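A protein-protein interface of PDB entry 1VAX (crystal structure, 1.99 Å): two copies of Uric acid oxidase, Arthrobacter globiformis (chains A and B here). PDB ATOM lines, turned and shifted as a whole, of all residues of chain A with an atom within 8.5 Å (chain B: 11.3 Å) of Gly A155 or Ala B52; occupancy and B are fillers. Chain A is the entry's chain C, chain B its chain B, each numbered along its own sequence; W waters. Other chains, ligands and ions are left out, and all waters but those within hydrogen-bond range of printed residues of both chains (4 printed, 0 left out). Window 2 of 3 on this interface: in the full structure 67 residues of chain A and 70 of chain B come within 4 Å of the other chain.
No position is printed for both chains.
Of the 14 pairs that touch across the chains among the printed residues, none has its exchanged pair printed and touching as well.
Water W3 lies within hydrogen-bond range of O of Pro A157 (2.6 Å), N of Ala B56 (2.8 Å) and OG1 of Thr B59 (3.1 Å).
Water W2 lies within hydrogen-bond range of the backbone carbonyl oxygen of Leu A210 (2.8 Å), the backbone NH of His A154 (2.9 Å) and the side-chain amide nitrogen of Asn B51 (3.2 Å).
Water W1 bridges OG1 of Thr B59 (2.9 Å) and N of Leu A164 (3.2 Å).
Water W4 lies within hydrogen-bond range of the backbone NH of Asn B51 (3.0 Å) and the backbone carbonyl oxygen of His A154 (3.0 Å).
Of the 12 printed residues of chain A, 7 touch a printed residue of chain B.
Of the 26 printed residues of chain B, 7 touch a printed residue of chain A.
Among the printed residues, 14 pairs touch across the chains.
Phe A153 touches just one residue of chain B: Asn B51 (3.5 Å).
Of chain B, only Asn B51 (3.0 Å) comes within 4 Å of His A154.
Printed residues of chain B within 4 Å of Gly A155: Asn B51 and Ala B52.
Printed residues of chain B within 4 Å of Pro A157: Asn B51, Ala B52, Val B54 and Trp B92.
Of the printed residues of chain A, Gly B49 touches Leu A210 (3.8 Å).
Printed residues of chain A within 4 Å of Asn B51: Phe A153, His A154, Gly A155, Phe A156, Pro A157 and Leu A210.
Ala B52 touches just these residues of chain A: Gly A155 and Pro A157.
Of the printed residues of chain A, Ala B56 touches Leu A164 (3.9 Å).
Of the printed residues of chain A, Trp B92 touches Pro A157 (3.8 Å).
The nearest residue of chain B that does not touch Gly A155 is Asp B50 (5.2 Å).
The nearest residue of chain A that does not touch Ala B52 is Phe A156 (4.9 Å).
The nearest printed residue of chain A that does not touch Gly B49 is His A154 (5.5 Å).
The backbone carbonyl oxygen (O) of His A154 lies within hydrogen-bond range of the side-chain amide nitrogen (ND2) of Asn B51, at 3.0 Å.
The side-chain amide nitrogen (ND2) of Asn B51 lies within hydrogen-bond range of the backbone carbonyl oxygen (O) of Leu A210.
The backbone carbonyl oxygen of Gly A155 lies close to the backbone carbonyl oxygen of Asn B51 (3.3 Å).
Among the printed residues, pairs that only touch across the chains: Pro A157 with Ala B52 (2.9 Å), Pro A157 with Val B54 (3.1 Å), Phe A156 with Val B54 (3.2 Å), Phe A156 with Asn B51 (3.2 Å), Pro A157 with Asn B51 (3.3 Å), Gly A155 with Ala B52 (3.5 Å), Phe A153 with Asn B51 (3.5 Å), Pro A157 with Trp B92 (3.8 Å), Leu A210 with Gly B49 (3.8 Å), Leu A164 with Ala B56 (3.9 Å) and Leu A210 with Ala B48 (3.95 Å).
O of Ala B44 lies within hydrogen-bond range of N of Gly B49.
OD1 of Asp B50 sits at hydrogen-bond distance from N of Ala B52 (3.3 Å).
The indole nitrogen (NE1) of Trp B92 lies within hydrogen-bond range of the backbone carbonyl oxygen (O) of His B53, at 2.7 Å.
A ring nitrogen (NE2) of His A154 sits at hydrogen-bond distance from the side-chain carboxylate of Glu A152.
N of Gly A155 lies within hydrogen-bond range of OE2 of Glu A166.
The guanidinium group (NH2) of Arg A158 is in hydrogen-bond range of the backbone carbonyl oxygen (O) of Leu A164 (2.9 Å).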
ATOM      1  N   GLU A 152      17.240  -5.659   4.532  1.00  0.00           N
ATOM      2  CA  GLU A 152      16.500  -5.724   5.781  1.00  0.00           C
ATOM      3  C   GLU A 152      17.258  -5.058   6.916  1.00  0.00           C
ATOM      4  O   GLU A 152      18.454  -4.780   6.800  1.00  0.00           O
ATOM      5  CB  GLU A 152      16.170  -7.183   6.132  1.00  0.00           C
ATOM      6  CG  GLU A 152      17.222  -8.211   5.753  1.00  0.00           C
ATOM      7  CD  GLU A 152      16.722  -9.643   5.922  1.00  0.00           C
ATOM      8  OE1 GLU A 152      16.315 -10.004   7.046  1.00  0.00           O
ATOM      9  OE2 GLU A 152      16.731 -10.410   4.933  1.00  0.00           O
ATOM     10  N   PHE A 153      16.549  -4.769   7.999  1.00  0.00           N
ATOM     11  CA  PHE A 153      17.163  -4.158   9.164  1.00  0.00           C
ATOM     12  C   PHE A 153      16.364  -4.527  10.400  1.00  0.00           C
ATOM     13  O   PHE A 153      15.251  -4.043  10.607  1.00  0.00           O
ATOM     14  CB  PHE A 153      17.227  -2.634   9.024  1.00  0.00           C
ATOM     15  CG  PHE A 153      18.047  -1.966  10.094  1.00  0.00           C
ATOM     16  CD1 PHE A 153      19.392  -2.286  10.255  1.00  0.00           C
ATOM     17  CD2 PHE A 153      17.475  -1.030  10.949  1.00  0.00           C
ATOM     18  CE1 PHE A 153      20.156  -1.685  11.252  1.00  0.00           C
ATOM     19  CE2 PHE A 153      18.230  -0.421  11.950  1.00  0.00           C
ATOM     20  CZ  PHE A 153      19.575  -0.751  12.102  1.00  0.00           C
ATOM     21  N   HIS A 154      16.946  -5.392  11.218  1.00  0.00           N
ATOM     22  CA  HIS A 154      16.299  -5.850  12.439  1.00  0.00           C
ATOM     23  C   HIS A 154      17.364  -6.302  13.423  1.00  0.00           C
ATOM     24  O   HIS A 154      18.536  -6.405  13.070  1.00  0.00           O
ATOM     25  CB  HIS A 154      15.354  -7.010  12.112  1.00  0.00           C
ATOM     26  CG  HIS A 154      15.987  -8.087  11.286  1.00  0.00           C
ATOM     27  ND1 HIS A 154      16.947  -8.942  11.784  1.00  0.00           N
ATOM     28  CD2 HIS A 154      15.818  -8.428   9.986  1.00  0.00           C
ATOM     29  CE1 HIS A 154      17.342  -9.763  10.828  1.00  0.00           C
ATOM     30  NE2 HIS A 154      16.673  -9.473   9.726  1.00  0.00           N
ATOM     31  N   GLY A 155      16.956  -6.563  14.661  1.00  0.00           N
ATOM     32  CA  GLY A 155      17.908  -7.005  15.659  1.00  0.00           C
ATOM     33  C   GLY A 155      18.687  -5.877  16.310  1.00  0.00           C
ATOM     34  O   GLY A 155      19.667  -6.126  17.015  1.00  0.00           O
ATOM     35  N   PHE A 156      18.270  -4.634  16.079  1.00  0.00           N
ATOM     36  CA  PHE A 156      18.952  -3.497  16.688  1.00  0.00           C
ATOM     37  C   PHE A 156      18.399  -3.240  18.087  1.00  0.00           C
ATOM     38  O   PHE A 156      17.263  -3.606  18.389  1.00  0.00           O
ATOM     39  CB  PHE A 156      18.798  -2.235  15.828  1.00  0.00           C
ATOM     40  CG  PHE A 156      17.379  -1.936  15.421  1.00  0.00           C
ATOM     41  CD1 PHE A 156      16.844  -2.486  14.263  1.00  0.00           C
ATOM     42  CD2 PHE A 156      16.584  -1.099  16.195  1.00  0.00           C
ATOM     43  CE1 PHE A 156      15.535  -2.205  13.879  1.00  0.00           C
ATOM     44  CE2 PHE A 156      15.270  -0.811  15.820  1.00  0.00           C
ATOM     45  CZ  PHE A 156      14.747  -1.365  14.661  1.00  0.00           C
ATOM     46  N   PRO A 157      19.199  -2.607  18.962  1.00  0.00           N
ATOM     47  CA  PRO A 157      18.791  -2.296  20.337  1.00  0.00           C
ATOM     48  C   PRO A 157      17.536  -1.422  20.386  1.00  0.00           C
ATOM     49  O   PRO A 157      17.318  -0.588  19.507  1.00  0.00           O
ATOM     50  CB  PRO A 157      20.005  -1.561  20.903  1.00  0.00           C
ATOM     51  CG  PRO A 157      21.141  -2.091  20.101  1.00  0.00           C
ATOM     52  CD  PRO A 157      20.579  -2.154  18.714  1.00  0.00           C
ATOM     53  N   ARG A 158      16.716  -1.607  21.415  1.00  0.00           N
ATOM     54  CA  ARG A 158      15.505  -0.807  21.558  1.00  0.00           C
ATOM     55  C   ARG A 158      15.448  -0.136  22.922  1.00  0.00           C
ATOM     56  O   ARG A 158      15.273  -0.802  23.944  1.00  0.00           O
ATOM     57  CB  ARG A 158      14.258  -1.675  21.376  1.00  0.00           C
ATOM     58  CG  ARG A 158      14.200  -2.444  20.067  1.00  0.00           C
ATOM     59  CD  ARG A 158      12.819  -3.067  19.868  1.00  0.00           C
ATOM     60  NE  ARG A 158      11.816  -2.079  19.473  1.00  0.00           N
ATOM     61  CZ  ARG A 158      11.739  -1.532  18.263  1.00  0.00           C
ATOM     62  NH1 ARG A 158      12.605  -1.877  17.320  1.00  0.00           N
ATOM     63  NH2 ARG A 158      10.794  -0.640  17.993  1.00  0.00           N
ATOM     64  N   LEU A 164      11.466   2.826  15.630  1.00  0.00           N
ATOM     65  CA  LEU A 164      11.644   2.156  14.344  1.00  0.00           C
ATOM     66  C   LEU A 164      11.239   0.682  14.390  1.00  0.00           C
ATOM     67  O   LEU A 164      11.632  -0.055  15.299  1.00  0.00           O
ATOM     68  CB  LEU A 164      13.105   2.265  13.890  1.00  0.00           C
ATOM     69  CG  LEU A 164      13.451   1.652  12.527  1.00  0.00           C
ATOM     70  CD1 LEU A 164      12.685   2.385  11.426  1.00  0.00           C
ATOM     71  CD2 LEU A 164      14.958   1.743  12.287  1.00  0.00           C
ATOM     72  N   GLN A 165      10.452   0.257  13.404  1.00  0.00           N
ATOM     73  CA  GLN A 165      10.005  -1.127  13.326  1.00  0.00           C
ATOM     74  C   GLN A 165      10.997  -1.966  12.535  1.00  0.00           C
ATOM     75  O   GLN A 165      11.562  -1.504  11.543  1.00  0.00           O
ATOM     76  CB  GLN A 165       8.626  -1.207  12.668  1.00  0.00           C
ATOM     77  CG  GLN A 165       7.517  -0.605  13.511  1.00  0.00           C
ATOM     78  CD  GLN A 165       7.461  -1.214  14.905  1.00  0.00           C
ATOM     79  OE1 GLN A 165       7.272  -2.423  15.060  1.00  0.00           O
ATOM     80  NE2 GLN A 165       7.630  -0.377  15.927  1.00  0.00           N
ATOM     81  N   GLU A 166      11.218  -3.198  12.981  1.00  0.00           N
ATOM     82  CA  GLU A 166      12.145  -4.080  12.288  1.00  0.00           C
ATOM     83  C   GLU A 166      11.542  -4.430  10.939  1.00  0.00           C
ATOM     84  O   GLU A 166      10.318  -4.464  10.789  1.00  0.00           O
ATOM     85  CB  GLU A 166      12.379  -5.364  13.087  1.00  0.00           C
ATOM     86  CG  GLU A 166      12.927  -5.153  14.487  1.00  0.00           C
ATOM     87  CD  GLU A 166      13.392  -6.452  15.120  1.00  0.00           C
ATOM     88  OE1 GLU A 166      12.647  -7.450  15.045  1.00  0.00           O
ATOM     89  OE2 GLU A 166      14.500  -6.477  15.696  1.00  0.00           O
ATOM     90  N   THR A 167      12.395  -4.692   9.954  1.00  0.00           N
ATOM     91  CA  THR A 167      11.909  -5.039   8.629  1.00  0.00           C
ATOM     92  C   THR A 167      12.801  -6.070   7.942  1.00  0.00           C
ATOM     93  O   THR A 167      14.002  -6.149   8.205  1.00  0.00           O
ATOM     94  CB  THR A 167      11.807  -3.786   7.727  1.00  0.00           C
ATOM     95  OG1 THR A 167      11.124  -4.129   6.519  1.00  0.00           O
ATOM     96  CG2 THR A 167      13.198  -3.258   7.374  1.00  0.00           C
ATOM     97  N   LEU A 210      21.880  -6.799   5.286  1.00  0.00           N
ATOM     98  CA  LEU A 210      21.263  -6.963   6.600  1.00  0.00           C
ATOM     99  C   LEU A 210      21.503  -5.654   7.340  1.00  0.00           C
ATOM    100  O   LEU A 210      20.995  -5.434   8.440  1.00  0.00           O
ATOM    101  CB  LEU A 210      21.907  -8.117   7.379  1.00  0.00           C
ATOM    102  CG  LEU A 210      21.617  -9.542   6.894  1.00  0.00           C
ATOM    103  CD1 LEU A 210      22.155 -10.546   7.912  1.00  0.00           C
ATOM    104  CD2 LEU A 210      20.117  -9.729   6.732  1.00  0.00           C
ATOM    105  N   TYR B  10      28.868   5.936  12.388  1.00  0.00           N
ATOM    106  CA  TYR B  10      27.578   6.037  11.712  1.00  0.00           C
ATOM    107  C   TYR B  10      26.579   6.769  12.599  1.00  0.00           C
ATOM    108  O   TYR B  10      26.727   6.808  13.821  1.00  0.00           O
ATOM    109  CB  TYR B  10      27.022   4.646  11.421  1.00  0.00           C
ATOM    110  CG  TYR B  10      26.374   4.049  12.645  1.00  0.00           C
ATOM    111  CD1 TYR B  10      27.138   3.711  13.763  1.00  0.00           C
ATOM    112  CD2 TYR B  10      24.990   3.904  12.722  1.00  0.00           C
ATOM    113  CE1 TYR B  10      26.542   3.252  14.930  1.00  0.00           C
ATOM    114  CE2 TYR B  10      24.380   3.444  13.888  1.00  0.00           C
ATOM    115  CZ  TYR B  10      25.163   3.123  14.988  1.00  0.00           C
ATOM    116  OH  TYR B  10      24.573   2.697  16.151  1.00  0.00           O
ATOM    117  N   LEU B  38      28.199   7.682  15.962  1.00  0.00           N
ATOM    118  CA  LEU B  38      28.785   6.931  17.066  1.00  0.00           C
ATOM    119  C   LEU B  38      29.996   6.115  16.637  1.00  0.00           C
ATOM    120  O   LEU B  38      30.104   5.696  15.485  1.00  0.00           O
ATOM    121  CB  LEU B  38      27.728   5.996  17.664  1.00  0.00           C
ATOM    122  CG  LEU B  38      26.364   6.626  17.977  1.00  0.00           C
ATOM    123  CD1 LEU B  38      25.440   5.573  18.553  1.00  0.00           C
ATOM    124  CD2 LEU B  38      26.525   7.786  18.958  1.00  0.00           C
ATOM    125  N   GLY B  40      32.781   2.932  18.143  1.00  0.00           N
ATOM    126  CA  GLY B  40      32.930   1.892  19.142  1.00  0.00           C
ATOM    127  C   GLY B  40      33.052   0.535  18.483  1.00  0.00           C
ATOM    128  O   GLY B  40      33.560   0.428  17.369  1.00  0.00           O
ATOM    129  N   ASP B  41      32.577  -0.507  19.158  1.00  0.00           N
ATOM    130  CA  ASP B  41      32.669  -1.849  18.602  1.00  0.00           C
ATOM    131  C   ASP B  41      31.481  -2.215  17.716  1.00  0.00           C
ATOM    132  O   ASP B  41      30.454  -2.702  18.197  1.00  0.00           O
ATOM    133  CB  ASP B  41      32.834  -2.869  19.732  1.00  0.00           C
ATOM    134  CG  ASP B  41      32.767  -4.295  19.238  1.00  0.00           C
ATOM    135  OD1 ASP B  41      33.185  -4.550  18.088  1.00  0.00           O
ATOM    136  OD2 ASP B  41      32.302  -5.163  20.006  1.00  0.00           O
ATOM    137  N   PHE B  42      31.642  -1.975  16.416  1.00  0.00           N
ATOM    138  CA  PHE B  42      30.613  -2.265  15.423  1.00  0.00           C
ATOM    139  C   PHE B  42      31.131  -3.280  14.418  1.00  0.00           C
ATOM    140  O   PHE B  42      30.635  -3.376  13.297  1.00  0.00           O
ATOM    141  CB  PHE B  42      30.204  -0.979  14.696  1.00  0.00           C
ATOM    142  CG  PHE B  42      29.670   0.081  15.612  1.00  0.00           C
ATOM    143  CD1 PHE B  42      30.280   1.326  15.685  1.00  0.00           C
ATOM    144  CD2 PHE B  42      28.573  -0.177  16.427  1.00  0.00           C
ATOM    145  CE1 PHE B  42      29.809   2.301  16.562  1.00  0.00           C
ATOM    146  CE2 PHE B  42      28.096   0.788  17.303  1.00  0.00           C
ATOM    147  CZ  PHE B  42      28.718   2.033  17.372  1.00  0.00           C
ATOM    148  N   GLU B  43      32.137  -4.038  14.841  1.00  0.00           N
ATOM    149  CA  GLU B  43      32.766  -5.064  14.016  1.00  0.00           C
ATOM    150  C   GLU B  43      31.749  -6.023  13.396  1.00  0.00           C
ATOM    151  O   GLU B  43      31.683  -6.172  12.173  1.00  0.00           O
ATOM    152  CB  GLU B  43      33.764  -5.852  14.871  1.00  0.00           C
ATOM    153  CG  GLU B  43      34.565  -6.911  14.131  1.00  0.00           C
ATOM    154  CD  GLU B  43      35.593  -6.315  13.186  1.00  0.00           C
ATOM    155  OE1 GLU B  43      36.318  -5.389  13.604  1.00  0.00           O
ATOM    156  OE2 GLU B  43      35.683  -6.781  12.030  1.00  0.00           O
ATOM    157  N   ALA B  44      30.957  -6.672  14.245  1.00  0.00           N
ATOM    158  CA  ALA B  44      29.961  -7.637  13.787  1.00  0.00           C
ATOM    159  C   ALA B  44      28.923  -7.042  12.842  1.00  0.00           C
ATOM    160  O   ALA B  44      28.391  -7.737  11.978  1.00  0.00           O
ATOM    161  CB  ALA B  44      29.267  -8.277  14.987  1.00  0.00           C
ATOM    162  N   ALA B  45      28.620  -5.761  13.009  1.00  0.00           N
ATOM    163  CA  ALA B  45      27.643  -5.118  12.144  1.00  0.00           C
ATOM    164  C   ALA B  45      28.161  -5.072  10.712  1.00  0.00           C
ATOM    165  O   ALA B  45      27.396  -5.241   9.766  1.00  0.00           O
ATOM    166  CB  ALA B  45      27.345  -3.710  12.638  1.00  0.00           C
ATOM    167  N   HIS B  46      29.467  -4.854  10.557  1.00  0.00           N
ATOM    168  CA  HIS B  46      30.070  -4.779   9.229  1.00  0.00           C
ATOM    169  C   HIS B  46      30.381  -6.141   8.614  1.00  0.00           C
ATOM    170  O   HIS B  46      30.047  -6.398   7.456  1.00  0.00           O
ATOM    171  CB  HIS B  46      31.362  -3.948   9.268  1.00  0.00           C
ATOM    172  CG  HIS B  46      31.143  -2.498   9.573  1.00  0.00           C
ATOM    173  ND1 HIS B  46      30.955  -2.026  10.856  1.00  0.00           N
ATOM    174  CD2 HIS B  46      31.052  -1.419   8.758  1.00  0.00           C
ATOM    175  CE1 HIS B  46      30.759  -0.718  10.817  1.00  0.00           C
ATOM    176  NE2 HIS B  46      30.813  -0.326   9.554  1.00  0.00           N
ATOM    177  N   THR B  47      31.018  -7.010   9.393  1.00  0.00           N
ATOM    178  CA  THR B  47      31.404  -8.331   8.906  1.00  0.00           C
ATOM    179  C   THR B  47      30.277  -9.356   8.827  1.00  0.00           C
ATOM    180  O   THR B  47      30.281 -10.205   7.942  1.00  0.00           O
ATOM    181  CB  THR B  47      32.540  -8.931   9.772  1.00  0.00           C
ATOM    182  OG1 THR B  47      32.083  -9.096  11.119  1.00  0.00           O
ATOM    183  CG2 THR B  47      33.756  -8.014   9.767  1.00  0.00           C
ATOM    184  N   ALA B  48      29.312  -9.277   9.739  1.00  0.00           N
ATOM    185  CA  ALA B  48      28.217 -10.241   9.751  1.00  0.00           C
ATOM    186  C   ALA B  48      26.827  -9.650   9.543  1.00  0.00           C
ATOM    187  O   ALA B  48      25.882 -10.374   9.224  1.00  0.00           O
ATOM    188  CB  ALA B  48      28.243 -11.020  11.058  1.00  0.00           C
ATOM    189  N   GLY B  49      26.693  -8.342   9.725  1.00  0.00           N
ATOM    190  CA  GLY B  49      25.389  -7.723   9.574  1.00  0.00           C
ATOM    191  C   GLY B  49      24.591  -7.883  10.859  1.00  0.00           C
ATOM    192  O   GLY B  49      23.364  -7.788  10.856  1.00  0.00           O
ATOM    193  N   ASP B  50      25.296  -8.144  11.957  1.00  0.00           N
ATOM    194  CA  ASP B  50      24.671  -8.305  13.268  1.00  0.00           C
ATOM    195  C   ASP B  50      24.470  -6.913  13.855  1.00  0.00           C
ATOM    196  O   ASP B  50      25.437  -6.226  14.181  1.00  0.00           O
ATOM    197  CB  ASP B  50      25.572  -9.147  14.175  1.00  0.00           C
ATOM    198  CG  ASP B  50      25.016  -9.297  15.576  1.00  0.00           C
ATOM    199  OD1 ASP B  50      23.798  -9.087  15.764  1.00  0.00           O
ATOM    200  OD2 ASP B  50      25.798  -9.638  16.491  1.00  0.00           O
ATOM    201  N   ASN B  51      23.209  -6.507  13.992  1.00  0.00           N
ATOM    202  CA  ASN B  51      22.872  -5.176  14.489  1.00  0.00           C
ATOM    203  C   ASN B  51      22.688  -5.034  15.997  1.00  0.00           C
ATOM    204  O   ASN B  51      22.134  -4.036  16.467  1.00  0.00           O
ATOM    205  CB  ASN B  51      21.616  -4.677  13.773  1.00  0.00           C
ATOM    206  CG  ASN B  51      21.787  -4.642  12.266  1.00  0.00           C
ATOM    207  OD1 ASN B  51      22.727  -4.032  11.757  1.00  0.00           O
ATOM    208  ND2 ASN B  51      20.883  -5.297  11.545  1.00  0.00           N
ATOM    209  N   ALA B  52      23.162  -6.015  16.755  1.00  0.00           N
ATOM    210  CA  ALA B  52      23.043  -5.979  18.211  1.00  0.00           C
ATOM    211  C   ALA B  52      23.615  -4.697  18.825  1.00  0.00           C
ATOM    212  O   ALA B  52      23.085  -4.184  19.810  1.00  0.00           O
ATOM    213  CB  ALA B  52      23.731  -7.202  18.817  1.00  0.00           C
ATOM    214  N   HIS B  53      24.695  -4.178  18.247  1.00  0.00           N
ATOM    215  CA  HIS B  53      25.315  -2.960  18.760  1.00  0.00           C
ATOM    216  C   HIS B  53      24.880  -1.712  18.000  1.00  0.00           C
ATOM    217  O   HIS B  53      25.251  -0.604  18.368  1.00  0.00           O
ATOM    218  CB  HIS B  53      26.846  -3.042  18.675  1.00  0.00           C
ATOM    219  CG  HIS B  53      27.461  -4.063  19.582  1.00  0.00           C
ATOM    220  ND1 HIS B  53      26.831  -4.540  20.710  1.00  0.00           N
ATOM    221  CD2 HIS B  53      28.676  -4.664  19.548  1.00  0.00           C
ATOM    222  CE1 HIS B  53      27.628  -5.390  21.332  1.00  0.00           C
ATOM    223  NE2 HIS B  53      28.754  -5.483  20.648  1.00  0.00           N
ATOM    224  N   VAL B  54      24.093  -1.883  16.947  1.00  0.00           N
ATOM    225  CA  VAL B  54      23.686  -0.733  16.151  1.00  0.00           C
ATOM    226  C   VAL B  54      22.464   0.038  16.638  1.00  0.00           C
ATOM    227  O   VAL B  54      21.323  -0.326  16.344  1.00  0.00           O
ATOM    228  CB  VAL B  54      23.455  -1.136  14.679  1.00  0.00           C
ATOM    229  CG1 VAL B  54      23.200   0.106  13.834  1.00  0.00           C
ATOM    230  CG2 VAL B  54      24.661  -1.897  14.150  1.00  0.00           C
ATOM    231  N   VAL B  55      22.711   1.105  17.390  1.00  0.00           N
ATOM    232  CA  VAL B  55      21.639   1.966  17.863  1.00  0.00           C
ATOM    233  C   VAL B  55      21.151   2.618  16.566  1.00  0.00           C
ATOM    234  O   VAL B  55      21.902   3.354  15.927  1.00  0.00           O
ATOM    235  CB  VAL B  55      22.187   3.051  18.825  1.00  0.00           C
ATOM    236  CG1 VAL B  55      21.071   3.978  19.260  1.00  0.00           C
ATOM    237  CG2 VAL B  55      22.827   2.390  20.044  1.00  0.00           C
ATOM    238  N   ALA B  56      19.916   2.322  16.167  1.00  0.00           N
ATOM    239  CA  ALA B  56      19.352   2.852  14.925  1.00  0.00           C
ATOM    240  C   ALA B  56      19.541   4.354  14.774  1.00  0.00           C
ATOM    241  O   ALA B  56      19.411   5.103  15.738  1.00  0.00           O
ATOM    242  CB  ALA B  56      17.866   2.504  14.835  1.00  0.00           C
ATOM    243  N   THR B  57      19.850   4.800  13.561  1.00  0.00           N
ATOM    244  CA  THR B  57      20.041   6.226  13.348  1.00  0.00           C
ATOM    245  C   THR B  57      18.713   6.928  13.626  1.00  0.00           C
ATOM    246  O   THR B  57      18.688   8.069  14.076  1.00  0.00           O
ATOM    247  CB  THR B  57      20.542   6.539  11.905  1.00  0.00           C
ATOM    248  OG1 THR B  57      19.556   6.149  10.943  1.00  0.00           O
ATOM    249  CG2 THR B  57      21.830   5.779  11.623  1.00  0.00           C
ATOM    250  N   THR B  59      16.717   6.185  15.955  1.00  0.00           N
ATOM    251  CA  THR B  59      16.693   6.361  17.407  1.00  0.00           C
ATOM    252  C   THR B  59      17.556   7.559  17.791  1.00  0.00           C
ATOM    253  O   THR B  59      17.213   8.326  18.693  1.00  0.00           O
ATOM    254  CB  THR B  59      17.228   5.106  18.135  1.00  0.00           C
ATOM    255  OG1 THR B  59      16.376   3.989  17.848  1.00  0.00           O
ATOM    256  CG2 THR B  59      17.265   5.332  19.646  1.00  0.00           C
ATOM    257  N   GLY B  89      25.427   5.547  27.789  1.00  0.00           N
ATOM    258  CA  GLY B  89      24.237   4.715  27.762  1.00  0.00           C
ATOM    259  C   GLY B  89      24.433   3.375  27.083  1.00  0.00           C
ATOM    260  O   GLY B  89      23.575   2.501  27.170  1.00  0.00           O
ATOM    261  N   PHE B  90      25.562   3.211  26.404  1.00  0.00           N
ATOM    262  CA  PHE B  90      25.865   1.970  25.706  1.00  0.00           C
ATOM    263  C   PHE B  90      27.336   1.619  25.928  1.00  0.00           C
ATOM    264  O   PHE B  90      28.228   2.415  25.628  1.00  0.00           O
ATOM    265  CB  PHE B  90      25.563   2.139  24.214  1.00  0.00           C
ATOM    266  CG  PHE B  90      24.149   2.561  23.931  1.00  0.00           C
ATOM    267  CD1 PHE B  90      23.118   1.627  23.915  1.00  0.00           C
ATOM    268  CD2 PHE B  90      23.838   3.902  23.724  1.00  0.00           C
ATOM    269  CE1 PHE B  90      21.800   2.022  23.699  1.00  0.00           C
ATOM    270  CE2 PHE B  90      22.519   4.306  23.506  1.00  0.00           C
ATOM    271  CZ  PHE B  90      21.501   3.363  23.495  1.00  0.00           C
ATOM    272  N   ASP B  91      27.582   0.424  26.455  1.00  0.00           N
ATOM    273  CA  ASP B  91      28.941  -0.022  26.742  1.00  0.00           C
ATOM    274  C   ASP B  91      29.827  -0.177  25.516  1.00  0.00           C
ATOM    275  O   ASP B  91      31.027   0.068  25.590  1.00  0.00           O
ATOM    276  CB  ASP B  91      28.911  -1.343  27.511  1.00  0.00           C
ATOM    277  CG  ASP B  91      28.125  -1.244  28.803  1.00  0.00           C
ATOM    278  OD1 ASP B  91      28.327  -0.254  29.540  1.00  0.00           O
ATOM    279  OD2 ASP B  91      27.314  -2.154  29.086  1.00  0.00           O
ATOM    280  N   TRP B  92      29.243  -0.585  24.393  1.00  0.00           N
ATOM    281  CA  TRP B  92      30.020  -0.777  23.171  1.00  0.00           C
ATOM    282  C   TRP B  92      30.320   0.524  22.430  1.00  0.00           C
ATOM    283  O   TRP B  92      31.152   0.544  21.522  1.00  0.00           O
ATOM    284  CB  TRP B  92      29.307  -1.763  22.241  1.00  0.00           C
ATOM    285  CG  TRP B  92      27.953  -1.318  21.819  1.00  0.00           C
ATOM    286  CD1 TRP B  92      27.657  -0.383  20.873  1.00  0.00           C
ATOM    287  CD2 TRP B  92      26.703  -1.771  22.347  1.00  0.00           C
ATOM    288  NE1 TRP B  92      26.296  -0.223  20.777  1.00  0.00           N
ATOM    289  CE2 TRP B  92      25.685  -1.063  21.671  1.00  0.00           C
ATOM    290  CE3 TRP B  92      26.342  -2.707  23.324  1.00  0.00           C
ATOM    291  CZ2 TRP B  92      24.328  -1.260  21.941  1.00  0.00           C
ATOM    292  CZ3 TRP B  92      24.989  -2.904  23.594  1.00  0.00           C
ATOM    293  CH2 TRP B  92      24.000  -2.182  22.902  1.00  0.00           C
ATOM    294  N   VAL B  93      29.637   1.602  22.808  1.00  0.00           N
ATOM    295  CA  VAL B  93      29.869   2.908  22.197  1.00  0.00           C
ATOM    296  C   VAL B  93      30.921   3.615  23.052  1.00  0.00           C
ATOM    297  O   VAL B  93      30.660   3.965  24.204  1.00  0.00           O
ATOM    298  CB  VAL B  93      28.581   3.760  22.162  1.00  0.00           C
ATOM    299  CG1 VAL B  93      28.894   5.160  21.623  1.00  0.00           C
ATOM    300  CG2 VAL B  93      27.533   3.077  21.283  1.00  0.00           C
HETATM  301  O   HOH W   1      13.884   4.740  16.602  1.00  0.00           O
HETATM  302  O   HOH W   2      18.909  -6.867   9.656  1.00  0.00           O
HETATM  303  O   HOH W   3      18.118   1.470  18.163  1.00  0.00           O
HETATM  304  O   HOH W   4      20.815  -8.230  13.861  1.00  0.00           O
